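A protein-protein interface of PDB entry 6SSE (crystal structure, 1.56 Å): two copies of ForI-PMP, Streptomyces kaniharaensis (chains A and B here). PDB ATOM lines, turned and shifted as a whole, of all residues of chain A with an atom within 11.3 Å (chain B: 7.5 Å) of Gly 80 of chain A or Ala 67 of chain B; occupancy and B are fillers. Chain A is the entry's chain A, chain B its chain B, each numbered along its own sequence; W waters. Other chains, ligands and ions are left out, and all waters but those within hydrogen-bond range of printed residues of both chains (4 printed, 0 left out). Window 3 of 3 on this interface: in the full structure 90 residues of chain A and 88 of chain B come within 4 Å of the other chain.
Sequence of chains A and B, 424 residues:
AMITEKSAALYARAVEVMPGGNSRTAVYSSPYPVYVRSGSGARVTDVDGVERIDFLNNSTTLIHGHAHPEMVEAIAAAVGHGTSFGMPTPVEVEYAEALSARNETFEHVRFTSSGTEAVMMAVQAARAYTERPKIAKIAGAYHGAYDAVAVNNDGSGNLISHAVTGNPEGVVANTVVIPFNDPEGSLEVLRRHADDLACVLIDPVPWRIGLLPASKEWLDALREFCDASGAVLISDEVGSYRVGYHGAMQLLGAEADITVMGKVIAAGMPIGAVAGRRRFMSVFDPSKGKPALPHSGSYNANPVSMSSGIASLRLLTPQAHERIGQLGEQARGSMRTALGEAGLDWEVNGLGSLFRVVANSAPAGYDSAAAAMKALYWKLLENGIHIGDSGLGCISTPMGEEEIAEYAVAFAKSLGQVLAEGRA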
ATOM      1  N   MET A  71      42.938 -14.621  12.812  1.00  0.00           N
ATOM      2  CA  MET A  71      42.324 -13.515  13.614  1.00  0.00           C
ATOM      3  C   MET A  71      41.391 -12.684  12.720  1.00  0.00           C
ATOM      4  O   MET A  71      40.223 -12.474  13.080  1.00  0.00           O
ATOM      5  CB  MET A  71      43.396 -12.601  14.213  1.00  0.00           C
ATOM      6  CG  MET A  71      44.322 -13.268  15.203  1.00  0.00           C
ATOM      7  SD  MET A  71      43.545 -13.742  16.751  1.00  0.00           S
ATOM      8  CE  MET A  71      42.744 -12.193  17.150  1.00  0.00           C
ATOM      9  N   VAL A  72      41.862 -12.284  11.545  1.00  0.00           N
ATOM     10  CA  VAL A  72      41.113 -11.447  10.586  1.00  0.00           C
ATOM     11  C   VAL A  72      39.828 -12.182  10.163  1.00  0.00           C
ATOM     12  O   VAL A  72      38.741 -11.572  10.240  1.00  0.00           O
ATOM     13  CB  VAL A  72      41.981 -11.113   9.385  1.00  0.00           C
ATOM     14  CG1 VAL A  72      41.160 -10.426   8.314  1.00  0.00           C
ATOM     15  CG2 VAL A  72      43.178 -10.289   9.796  1.00  0.00           C
ATOM     16  N   GLU A  73      39.919 -13.483   9.902  1.00  0.00           N
ATOM     17  CA  GLU A  73      38.716 -14.223   9.470  1.00  0.00           C
ATOM     18  C   GLU A  73      37.682 -14.182  10.593  1.00  0.00           C
ATOM     19  O   GLU A  73      36.476 -14.009  10.304  1.00  0.00           O
ATOM     20  CB  GLU A  73      39.126 -15.662   9.197  1.00  0.00           C
ATOM     21  CG  GLU A  73      37.970 -16.496   8.673  1.00  0.00           C
ATOM     22  CD  GLU A  73      38.446 -17.826   8.081  1.00  0.00           C
ATOM     23  OE1 GLU A  73      39.459 -18.382   8.599  1.00  0.00           O
ATOM     24  OE2 GLU A  73      37.839 -18.284   7.078  1.00  0.00           O
ATOM     25  N   ALA A  74      38.113 -14.491  11.826  1.00  0.00           N
ATOM     26  CA  ALA A  74      37.186 -14.592  12.980  1.00  0.00           C
ATOM     27  C   ALA A  74      36.570 -13.208  13.258  1.00  0.00           C
ATOM     28  O   ALA A  74      35.352 -13.108  13.543  1.00  0.00           O
ATOM     29  CB  ALA A  74      37.909 -15.093  14.186  1.00  0.00           C
ATOM     30  N   ILE A  75      37.376 -12.187  13.268  1.00  0.00           N
ATOM     31  CA  ILE A  75      36.912 -10.793  13.585  1.00  0.00           C
ATOM     32  C   ILE A  75      35.960 -10.304  12.488  1.00  0.00           C
ATOM     33  O   ILE A  75      34.852  -9.822  12.804  1.00  0.00           O
ATOM     34  CB  ILE A  75      38.093  -9.849  13.828  1.00  0.00           C
ATOM     35  CG1 ILE A  75      38.886 -10.233  15.070  1.00  0.00           C
ATOM     36  CG2 ILE A  75      37.647  -8.389  13.876  1.00  0.00           C
ATOM     37  CD1 ILE A  75      40.289  -9.611  15.144  1.00  0.00           C
ATOM     38  N   ALA A  76      36.320 -10.461  11.214  1.00  0.00           N
ATOM     39  CA  ALA A  76      35.458 -10.012  10.111  1.00  0.00           C
ATOM     40  C   ALA A  76      34.122 -10.781  10.091  1.00  0.00           C
ATOM     41  O   ALA A  76      33.108 -10.162   9.832  1.00  0.00           O
ATOM     42  CB  ALA A  76      36.203 -10.118   8.821  1.00  0.00           C
ATOM     43  N   ALA A  77      34.093 -12.071  10.431  1.00  0.00           N
ATOM     44  CA  ALA A  77      32.835 -12.837  10.463  1.00  0.00           C
ATOM     45  C   ALA A  77      31.968 -12.269  11.585  1.00  0.00           C
ATOM     46  O   ALA A  77      30.745 -12.046  11.372  1.00  0.00           O
ATOM     47  CB  ALA A  77      33.100 -14.317  10.636  1.00  0.00           C
ATOM     48  N   ALA A  78      32.569 -11.988  12.739  1.00  0.00           N
ATOM     49  CA  ALA A  78      31.780 -11.425  13.869  1.00  0.00           C
ATOM     50  C   ALA A  78      31.218 -10.052  13.462  1.00  0.00           C
ATOM     51  O   ALA A  78      30.033  -9.783  13.732  1.00  0.00           O
ATOM     52  CB  ALA A  78      32.630 -11.303  15.117  1.00  0.00           C
ATOM     53  N   VAL A  79      32.026  -9.175  12.906  1.00  0.00           N
ATOM     54  CA  VAL A  79      31.577  -7.820  12.424  1.00  0.00           C
ATOM     55  C   VAL A  79      30.332  -7.965  11.527  1.00  0.00           C
ATOM     56  O   VAL A  79      29.410  -7.162  11.668  1.00  0.00           O
ATOM     57  CB  VAL A  79      32.699  -7.071  11.700  1.00  0.00           C
ATOM     58  CG1 VAL A  79      32.211  -5.797  11.039  1.00  0.00           C
ATOM     59  CG2 VAL A  79      33.804  -6.739  12.707  1.00  0.00           C
ATOM     60  N   GLY A  80      30.336  -8.953  10.647  1.00  0.00           N
ATOM     61  CA  GLY A  80      29.229  -9.116   9.675  1.00  0.00           C
ATOM     62  C   GLY A  80      27.901  -9.418  10.378  1.00  0.00           C
ATOM     63  O   GLY A  80      26.836  -9.240   9.744  1.00  0.00           O
ATOM     64  N   HIS A  81      27.948 -10.061  11.540  1.00  0.00           N
ATOM     65  CA  HIS A  81      26.753 -10.457  12.326  1.00  0.00           C
ATOM     66  C   HIS A  81      26.312  -9.349  13.292  1.00  0.00           C
ATOM     67  O   HIS A  81      25.206  -9.479  13.849  1.00  0.00           O
ATOM     68  CB  HIS A  81      27.003 -11.739  13.088  1.00  0.00           C
ATOM     69  CG  HIS A  81      27.013 -12.940  12.195  1.00  0.00           C
ATOM     70  ND1 HIS A  81      28.168 -13.639  11.919  1.00  0.00           N
ATOM     71  CD2 HIS A  81      26.012 -13.539  11.514  1.00  0.00           C
ATOM     72  CE1 HIS A  81      27.881 -14.648  11.108  1.00  0.00           C
ATOM     73  NE2 HIS A  81      26.563 -14.592  10.832  1.00  0.00           N
ATOM     74  N   GLY A  82      27.102  -8.304  13.498  1.00  0.00           N
ATOM     75  CA  GLY A  82      26.722  -7.198  14.382  1.00  0.00           C
ATOM     76  C   GLY A  82      27.866  -6.942  15.366  1.00  0.00           C
ATOM     77  O   GLY A  82      28.346  -7.897  15.970  1.00  0.00           O
ATOM     78  N   THR A  83      28.280  -5.699  15.500  1.00  0.00           N
ATOM     79  CA  THR A  83      29.500  -5.341  16.284  1.00  0.00           C
ATOM     80  C   THR A  83      29.201  -5.377  17.784  1.00  0.00           C
ATOM     81  O   THR A  83      30.121  -5.685  18.539  1.00  0.00           O
ATOM     82  CB  THR A  83      30.086  -4.022  15.811  1.00  0.00           C
ATOM     83  OG1 THR A  83      29.124  -3.024  16.060  1.00  0.00           O
ATOM     84  CG2 THR A  83      30.480  -4.105  14.345  1.00  0.00           C
ATOM     85  N   SER A  84      28.005  -4.948  18.210  1.00  0.00           N
ATOM     86  CA  SER A  84      27.644  -4.921  19.644  1.00  0.00           C
ATOM     87  C   SER A  84      26.133  -4.936  19.758  1.00  0.00           C
ATOM     88  O   SER A  84      25.440  -4.599  18.799  1.00  0.00           O
ATOM     89  CB  SER A  84      28.285  -3.765  20.384  1.00  0.00           C
ATOM     90  OG  SER A  84      27.936  -2.475  19.860  1.00  0.00           O
ATOM     91  N   PHE A  85      25.681  -5.457  20.861  1.00  0.00           N
ATOM     92  CA  PHE A  85      24.235  -5.710  21.142  1.00  0.00           C
ATOM     93  C   PHE A  85      23.965  -5.317  22.592  1.00  0.00           C
ATOM     94  O   PHE A  85      24.844  -5.393  23.477  1.00  0.00           O
ATOM     95  CB  PHE A  85      23.903  -7.193  20.973  1.00  0.00           C
ATOM     96  CG  PHE A  85      24.096  -7.716  19.573  1.00  0.00           C
ATOM     97  CD1 PHE A  85      23.028  -7.685  18.694  1.00  0.00           C
ATOM     98  CD2 PHE A  85      25.262  -8.291  19.145  1.00  0.00           C
ATOM     99  CE1 PHE A  85      23.151  -8.183  17.410  1.00  0.00           C
ATOM    100  CE2 PHE A  85      25.398  -8.764  17.846  1.00  0.00           C
ATOM    101  CZ  PHE A  85      24.334  -8.721  16.979  1.00  0.00           C
ATOM    102  N   VAL A  91      29.047 -16.105  21.989  1.00  0.00           N
ATOM    103  CA  VAL A  91      30.548 -16.055  21.994  1.00  0.00           C
ATOM    104  C   VAL A  91      31.038 -15.511  23.327  1.00  0.00           C
ATOM    105  O   VAL A  91      32.166 -15.841  23.715  1.00  0.00           O
ATOM    106  CB  VAL A  91      31.186 -15.249  20.842  1.00  0.00           C
ATOM    107  CG1 VAL A  91      31.221 -16.024  19.539  1.00  0.00           C
ATOM    108  CG2 VAL A  91      30.573 -13.863  20.702  1.00  0.00           C
ATOM    109  N   MET A 269      42.085  -6.478  19.600  1.00  0.00           N
ATOM    110  CA  MET A 269      40.786  -5.769  19.743  1.00  0.00           C
ATOM    111  C   MET A 269      40.566  -5.369  21.192  1.00  0.00           C
ATOM    112  O   MET A 269      41.131  -5.964  22.123  1.00  0.00           O
ATOM    113  CB  MET A 269      39.631  -6.672  19.313  1.00  0.00           C
ATOM    114  CG  MET A 269      39.675  -7.043  17.834  1.00  0.00           C
ATOM    115  SD  MET A 269      39.660  -5.630  16.707  1.00  0.00           S
ATOM    116  CE  MET A 269      38.042  -4.956  17.031  1.00  0.00           C
ATOM    117  N   ASN A 302      31.451  -7.544  23.945  1.00  0.00           N
ATOM    118  CA  ASN A 302      30.954  -7.389  22.566  1.00  0.00           C
ATOM    119  C   ASN A 302      31.489  -8.569  21.731  1.00  0.00           C
ATOM    120  O   ASN A 302      32.623  -9.014  21.906  1.00  0.00           O
ATOM    121  CB  ASN A 302      31.311  -6.024  21.974  1.00  0.00           C
ATOM    122  CG  ASN A 302      32.751  -5.947  21.568  1.00  0.00           C
ATOM    123  OD1 ASN A 302      33.088  -6.428  20.460  1.00  0.00           O
ATOM    124  ND2 ASN A 302      33.604  -5.378  22.433  1.00  0.00           N
ATOM    125  N   PRO A 303      30.713  -9.064  20.740  1.00  0.00           N
ATOM    126  CA  PRO A 303      31.098 -10.302  20.044  1.00  0.00           C
ATOM    127  C   PRO A 303      32.311 -10.141  19.141  1.00  0.00           C
ATOM    128  O   PRO A 303      32.923 -11.168  18.842  1.00  0.00           O
ATOM    129  CB  PRO A 303      29.793 -10.680  19.291  1.00  0.00           C
ATOM    130  CG  PRO A 303      29.079  -9.353  19.131  1.00  0.00           C
ATOM    131  CD  PRO A 303      29.333  -8.655  20.452  1.00  0.00           C
ATOM    132  N   VAL A 304      32.688  -8.913  18.808  1.00  0.00           N
ATOM    133  CA  VAL A 304      33.920  -8.744  17.969  1.00  0.00           C
ATOM    134  C   VAL A 304      35.130  -9.016  18.872  1.00  0.00           C
ATOM    135  O   VAL A 304      36.028  -9.811  18.476  1.00  0.00           O
ATOM    136  CB  VAL A 304      33.955  -7.378  17.271  1.00  0.00           C
ATOM    137  CG1 VAL A 304      35.213  -7.303  16.421  1.00  0.00           C
ATOM    138  CG2 VAL A 304      32.717  -7.199  16.433  1.00  0.00           C
ATOM    139  N   SER A 305      35.170  -8.397  20.038  1.00  0.00           N
ATOM    140  CA  SER A 305      36.277  -8.612  21.000  1.00  0.00           C
ATOM    141  C   SER A 305      36.261 -10.060  21.506  1.00  0.00           C
ATOM    142  O   SER A 305      37.352 -10.671  21.590  1.00  0.00           O
ATOM    143  CB  SER A 305      36.257  -7.637  22.123  1.00  0.00           C
ATOM    144  OG  SER A 305      36.456  -6.307  21.665  1.00  0.00           O
ATOM    145  N   SER A 307      35.232 -12.668  19.761  1.00  0.00           N
ATOM    146  CA  SER A 307      35.657 -13.502  18.621  1.00  0.00           C
ATOM    147  C   SER A 307      37.177 -13.383  18.478  1.00  0.00           C
ATOM    148  O   SER A 307      37.837 -14.390  18.202  1.00  0.00           O
ATOM    149  CB  SER A 307      34.916 -13.176  17.367  1.00  0.00           C
ATOM    150  OG  SER A 307      33.524 -13.506  17.533  1.00  0.00           O
ATOM    151  N   SER B  38      22.658 -12.505  15.974  1.00  0.00           N
ATOM    152  CA  SER B  38      22.933 -11.672  14.797  1.00  0.00           C
ATOM    153  C   SER B  38      21.975 -10.527  14.719  1.00  0.00           C
ATOM    154  O   SER B  38      20.848 -10.580  15.336  1.00  0.00           O
ATOM    155  CB  SER B  38      22.978 -12.451  13.498  1.00  0.00           C
ATOM    156  OG  SER B  38      21.657 -12.920  13.206  1.00  0.00           O
ATOM    157  N   GLY B  39      22.399  -9.510  14.010  1.00  0.00           N
ATOM    158  CA  GLY B  39      21.503  -8.392  13.684  1.00  0.00           C
ATOM    159  C   GLY B  39      21.684  -8.021  12.244  1.00  0.00           C
ATOM    160  O   GLY B  39      22.817  -8.109  11.730  1.00  0.00           O
ATOM    161  N   SER B  40      20.633  -7.513  11.636  1.00  0.00           N
ATOM    162  CA  SER B  40      20.665  -6.980  10.244  1.00  0.00           C
ATOM    163  C   SER B  40      19.704  -5.809  10.142  1.00  0.00           C
ATOM    164  O   SER B  40      18.460  -6.012  10.376  1.00  0.00           O
ATOM    165  CB  SER B  40      20.382  -8.107   9.267  1.00  0.00           C
ATOM    166  OG  SER B  40      20.491  -7.626   7.942  1.00  0.00           O
ATOM    167  N   GLY B  41      20.206  -4.618   9.886  1.00  0.00           N
ATOM    168  CA  GLY B  41      19.386  -3.413   9.758  1.00  0.00           C
ATOM    169  C   GLY B  41      18.752  -3.075  11.081  1.00  0.00           C
ATOM    170  O   GLY B  41      19.479  -2.909  12.070  1.00  0.00           O
ATOM    171  N   ARG B  43      16.755  -5.100  12.782  1.00  0.00           N
ATOM    172  CA  ARG B  43      16.277  -6.345  13.405  1.00  0.00           C
ATOM    173  C   ARG B  43      17.388  -7.184  14.007  1.00  0.00           C
ATOM    174  O   ARG B  43      18.524  -7.203  13.469  1.00  0.00           O
ATOM    175  CB  ARG B  43      15.486  -7.156  12.376  1.00  0.00           C
ATOM    176  CG  ARG B  43      14.177  -6.471  12.008  1.00  0.00           C
ATOM    177  CD  ARG B  43      13.531  -7.013  10.738  1.00  0.00           C
ATOM    178  NE  ARG B  43      12.169  -6.474  10.689  1.00  0.00           N
ATOM    179  CZ  ARG B  43      11.833  -5.285  10.188  1.00  0.00           C
ATOM    180  NH1 ARG B  43      12.734  -4.471   9.672  1.00  0.00           N
ATOM    181  NH2 ARG B  43      10.567  -4.888  10.251  1.00  0.00           N
ATOM    182  N   LEU B  62      23.732   2.137  18.542  1.00  0.00           N
ATOM    183  CA  LEU B  62      23.718   1.726  17.116  1.00  0.00           C
ATOM    184  C   LEU B  62      22.826   2.675  16.343  1.00  0.00           C
ATOM    185  O   LEU B  62      21.720   2.236  15.871  1.00  0.00           O
ATOM    186  CB  LEU B  62      23.294   0.279  16.946  1.00  0.00           C
ATOM    187  CG  LEU B  62      24.034  -0.761  17.792  1.00  0.00           C
ATOM    188  CD1 LEU B  62      23.373  -2.110  17.675  1.00  0.00           C
ATOM    189  CD2 LEU B  62      25.494  -0.864  17.306  1.00  0.00           C
ATOM    190  N   HIS B  64      23.061   3.585  13.385  1.00  0.00           N
ATOM    191  CA  HIS B  64      22.846   3.050  12.032  1.00  0.00           C
ATOM    192  C   HIS B  64      22.366   1.615  12.101  1.00  0.00           C
ATOM    193  O   HIS B  64      22.515   0.901  11.111  1.00  0.00           O
ATOM    194  CB  HIS B  64      24.162   3.221  11.246  1.00  0.00           C
ATOM    195  CG  HIS B  64      24.555   4.629  11.185  1.00  0.00           C
ATOM    196  ND1 HIS B  64      23.677   5.619  10.721  1.00  0.00           N
ATOM    197  CD2 HIS B  64      25.718   5.244  11.494  1.00  0.00           C
ATOM    198  CE1 HIS B  64      24.275   6.786  10.817  1.00  0.00           C
ATOM    199  NE2 HIS B  64      25.540   6.574  11.261  1.00  0.00           N
ATOM    200  N   GLY B  65      21.812   1.151  13.244  1.00  0.00           N
ATOM    201  CA  GLY B  65      21.395  -0.243  13.351  1.00  0.00           C
ATOM    202  C   GLY B  65      22.514  -1.238  13.181  1.00  0.00           C
ATOM    203  O   GLY B  65      23.710  -0.944  13.528  1.00  0.00           O
ATOM    204  N   HIS B  66      22.126  -2.446  12.877  1.00  0.00           N
ATOM    205  CA  HIS B  66      22.989  -3.630  12.965  1.00  0.00           C
ATOM    206  C   HIS B  66      23.669  -3.907  11.626  1.00  0.00           C
ATOM    207  O   HIS B  66      22.978  -3.983  10.587  1.00  0.00           O
ATOM    208  CB  HIS B  66      22.205  -4.842  13.429  1.00  0.00           C
ATOM    209  CG  HIS B  66      21.644  -4.670  14.800  1.00  0.00           C
ATOM    210  ND1 HIS B  66      22.352  -5.076  15.934  1.00  0.00           N
ATOM    211  CD2 HIS B  66      20.501  -4.056  15.223  1.00  0.00           C
ATOM    212  CE1 HIS B  66      21.572  -4.836  16.981  1.00  0.00           C
ATOM    213  NE2 HIS B  66      20.484  -4.159  16.579  1.00  0.00           N
ATOM    214  N   ALA B  67      24.978  -4.068  11.657  1.00  0.00           N
ATOM    215  CA  ALA B  67      25.719  -4.526  10.456  1.00  0.00           C
ATOM    216  C   ALA B  67      25.320  -3.706   9.245  1.00  0.00           C
ATOM    217  O   ALA B  67      25.077  -4.287   8.160  1.00  0.00           O
ATOM    218  CB  ALA B  67      25.510  -5.984  10.223  1.00  0.00           C
ATOM    219  N   HIS B  68      25.325  -2.398   9.381  1.00  0.00           N
ATOM    220  CA  HIS B  68      25.083  -1.502   8.225  1.00  0.00           C
ATOM    221  C   HIS B  68      26.175  -1.818   7.210  1.00  0.00           C
ATOM    222  O   HIS B  68      27.348  -1.866   7.551  1.00  0.00           O
ATOM    223  CB  HIS B  68      25.177  -0.068   8.676  1.00  0.00           C
ATOM    224  CG  HIS B  68      24.790   0.929   7.636  1.00  0.00           C
ATOM    225  ND1 HIS B  68      25.556   1.144   6.468  1.00  0.00           N
ATOM    226  CD2 HIS B  68      23.730   1.781   7.554  1.00  0.00           C
ATOM    227  CE1 HIS B  68      25.000   2.118   5.777  1.00  0.00           C
ATOM    228  NE2 HIS B  68      23.861   2.547   6.407  1.00  0.00           N
ATOM    229  N   PRO B  69      25.827  -2.088   5.942  1.00  0.00           N
ATOM    230  CA  PRO B  69      26.832  -2.494   4.964  1.00  0.00           C
ATOM    231  C   PRO B  69      28.047  -1.570   4.876  1.00  0.00           C
ATOM    232  O   PRO B  69      29.156  -2.063   4.594  1.00  0.00           O
ATOM    233  CB  PRO B  69      26.041  -2.574   3.630  1.00  0.00           C
ATOM    234  CG  PRO B  69      24.743  -1.841   3.896  1.00  0.00           C
ATOM    235  CD  PRO B  69      24.473  -2.070   5.378  1.00  0.00           C
ATOM    236  N   GLU B  70      27.826  -0.252   4.946  1.00  0.00           N
ATOM    237  CA  GLU B  70      28.946   0.705   4.841  1.00  0.00           C
ATOM    238  C   GLU B  70      29.797   0.682   6.104  1.00  0.00           C
ATOM    239  O   GLU B  70      31.012   0.900   6.013  1.00  0.00           O
ATOM    240  CB  GLU B  70      28.471   2.104   4.467  1.00  0.00           C
ATOM    241  CG  GLU B  70      27.855   2.089   3.041  1.00  0.00           C
ATOM    242  CD  GLU B  70      27.206   3.385   2.584  1.00  0.00           C
ATOM    243  OE1 GLU B  70      27.958   4.288   2.307  1.00  0.00           O
ATOM    244  OE2 GLU B  70      25.950   3.511   2.649  1.00  0.00           O
ATOM    245  N   MET B  71      29.188   0.442   7.261  1.00  0.00           N
ATOM    246  CA  MET B  71      29.936   0.251   8.543  1.00  0.00           C
ATOM    247  C   MET B  71      30.773  -1.032   8.465  1.00  0.00           C
ATOM    248  O   MET B  71      31.996  -0.974   8.720  1.00  0.00           O
ATOM    249  CB  MET B  71      28.986   0.173   9.745  1.00  0.00           C
ATOM    250  CG  MET B  71      28.187   1.449  10.010  1.00  0.00           C
ATOM    251  SD  MET B  71      29.200   2.867  10.490  1.00  0.00           S
ATOM    252  CE  MET B  71      30.180   2.119  11.785  1.00  0.00           C
ATOM    253  N   VAL B  72      30.172  -2.131   8.031  1.00  0.00           N
ATOM    254  CA  VAL B  72      30.835  -3.457   7.904  1.00  0.00           C
ATOM    255  C   VAL B  72      32.026  -3.337   6.957  1.00  0.00           C
ATOM    256  O   VAL B  72      33.124  -3.769   7.318  1.00  0.00           O
ATOM    257  CB  VAL B  72      29.849  -4.498   7.415  1.00  0.00           C
ATOM    258  CG1 VAL B  72      30.527  -5.784   7.002  1.00  0.00           C
ATOM    259  CG2 VAL B  72      28.764  -4.694   8.446  1.00  0.00           C
ATOM    260  N   GLU B  73      31.841  -2.641   5.827  1.00  0.00           N
ATOM    261  CA  GLU B  73      32.942  -2.524   4.869  1.00  0.00           C
ATOM    262  C   GLU B  73      34.124  -1.808   5.539  1.00  0.00           C
ATOM    263  O   GLU B  73      35.259  -2.271   5.383  1.00  0.00           O
ATOM    264  CB  GLU B  73      32.453  -1.727   3.655  1.00  0.00           C
ATOM    265  CG  GLU B  73      33.596  -1.483   2.711  1.00  0.00           C
ATOM    266  CD  GLU B  73      33.384  -0.505   1.571  1.00  0.00           C
ATOM    267  OE1 GLU B  73      32.283   0.005   1.401  1.00  0.00           O
ATOM    268  OE2 GLU B  73      34.393  -0.232   0.908  1.00  0.00           O
ATOM    269  N   ILE B  75      34.845  -1.173   8.731  1.00  0.00           N
ATOM    270  CA  ILE B  75      35.436  -1.932   9.893  1.00  0.00           C
ATOM    271  C   ILE B  75      36.244  -3.140   9.405  1.00  0.00           C
ATOM    272  O   ILE B  75      37.439  -3.324   9.836  1.00  0.00           O
ATOM    273  CB  ILE B  75      34.340  -2.272  10.905  1.00  0.00           C
ATOM    274  CG1 ILE B  75      33.712  -1.014  11.498  1.00  0.00           C
ATOM    275  CG2 ILE B  75      34.831  -3.225  11.961  1.00  0.00           C
ATOM    276  CD1 ILE B  75      32.384  -1.249  12.189  1.00  0.00           C
ATOM    277  N   ALA B  76      35.690  -3.974   8.529  1.00  0.00           N
ATOM    278  CA  ALA B  76      36.316  -5.248   8.168  1.00  0.00           C
ATOM    279  C   ALA B  76      37.580  -4.951   7.336  1.00  0.00           C
ATOM    280  O   ALA B  76      38.567  -5.633   7.461  1.00  0.00           O
ATOM    281  CB  ALA B  76      35.364  -6.140   7.436  1.00  0.00           C
ATOM    282  N   ALA B 267      29.129   4.184  16.472  1.00  0.00           N
ATOM    283  CA  ALA B 267      27.949   3.412  16.053  1.00  0.00           C
ATOM    284  C   ALA B 267      28.204   1.909  16.149  1.00  0.00           C
ATOM    285  O   ALA B 267      27.625   1.148  15.361  1.00  0.00           O
ATOM    286  CB  ALA B 267      27.456   3.822  14.685  1.00  0.00           C
ATOM    287  N   PRO B 398      18.217   2.712   9.717  1.00  0.00           N
ATOM    288  CA  PRO B 398      17.532   1.755   8.863  1.00  0.00           C
ATOM    289  C   PRO B 398      16.000   1.743   8.987  1.00  0.00           C
ATOM    290  O   PRO B 398      15.341   1.162   8.142  1.00  0.00           O
ATOM    291  CB  PRO B 398      18.093   0.376   9.193  1.00  0.00           C
ATOM    292  CG  PRO B 398      19.404   0.698   9.902  1.00  0.00           C
ATOM    293  CD  PRO B 398      19.203   2.042  10.577  1.00  0.00           C
HETATM  294  O   HOH W   1      27.931  -1.304  14.177  1.00  0.00           O
HETATM  295  O   HOH W   2      26.359  -3.717  14.154  1.00  0.00           O
HETATM  296  O   HOH W   3      24.160  -9.325   9.848  1.00  0.00           O
HETATM  297  O   HOH W   4      25.030  -5.041  16.084  1.00  0.00           O
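Positions printed for both chains: 71, 72, 73, 75 and 76.
Among the printed residues, merely in contact across the chains: His 81 of chain A with Ser 38 of chain B, Ser 84 of chain A with Leu 62 of chain B, Phe 85 of chain A with His 66 of chain B, Gly 80 of chain A with Ala 67 of chain B, Phe 85 of chain A with Gly 39 of chain B, Phe 85 of chain A with Ser 38 of chain B and Val 79 of chain A with Ile 75 of chain B.
Gly 80 of chain A touches just one residue of chain B: Ala 67.
Of the printed residues of chain A, Ala 67 of chain B touches Gly 80 (3.5 Å).
Of chain A, only His 81 (2.8 Å) and Phe 85 (3.6 Å) come within 4 Å of Gly 39 of chain B.
No residue of chain A comes within 4 Å of Ser 40 of chain B.
No residue of chain A comes within 4 Å of Gly 41 of chain B.
No residue of chain A comes within 4 Å of Gly 65 of chain B.
His 66 of chain B touches just one residue of chain A: Phe 85.
No residue of chain A comes within 4 Å of Val 72 of chain B.
Printed residues of chain B within 4 Å of Val 79 of chain A: Ile 75.
Of the printed residues of chain A, Ser 38 of chain B touches His 81 (3.3 Å) and Phe 85 (3.7 Å).
Of the printed residues of chain B, His 81 of chain A touches Ser 38 and Gly 39.
Printed residues of chain B within 4 Å of Phe 85 of chain A: Ser 38 (3.7 Å), Gly 39 (3.6 Å) and His 66 (3.5 Å).
Glu 73 of chain B touches none of the printed residues of chain A.
Ile 75 of chain A touches none of the printed residues of chain B.
The nearest printed residue of chain A that does not touch Ala 67 of chain B is Gly 82 of chain A (4.3 Å).
Of the 22 printed residues of chain A, 5 touch a printed residue of chain B.
Printed residues of chain A that touch a printed residue of chain B: Val 79, Gly 80, His 81, Ser 84 and Phe 85.
Hydrophobic or aromatic side chains of chain A within 4 Å of the printed part of chain B: Val 79, His 81 and Phe 85.
Along chain A the printed residues that touch a printed residue of chain B span positions 79 to 85.
Hydrophobic or aromatic side chains of chain B within 4 Å of the printed part of chain A: Leu 62, His 66, Ala 67 and Ile 75.
Among the printed residues, no Asp or Glu carboxylate lies within 4 Å of a Lys or Arg side-chain nitrogen of the other chain.
The backbone NH (N) of Gly 39 of chain B lies within hydrogen-bond range of the backbone carbonyl oxygen (O) of His 81 of chain A, at 2.8 Å.
A ring nitrogen (ND1) of His 81 of chain A sits at hydrogen-bond distance from the backbone carbonyl oxygen of Ala 77 of chain A (3.1 Å).
The backbone NH of His 66 of chain B is in hydrogen-bond range of the backbone carbonyl oxygen of Gly 41 of chain B.
Water W3 bridges O of Gly 39 of chain B (2.6 Å) and O of Gly 80 of chain A (2.7 Å).
Water W4 lies within hydrogen-bond range of ND1 of His 66 of chain B (2.7 Å), O of Ser 84 of chain A (2.8 Å) and N of Thr 83 of chain A (3.4 Å).
Water W1 bridges O of Ala 267 of chain B and OG1 of Thr 83 of chain A.
Water W2 lies within hydrogen-bond range of the backbone NH of Ala 67 of chain B (2.9 Å) and the backbone NH of Thr 83 of chain A (3.1 Å).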
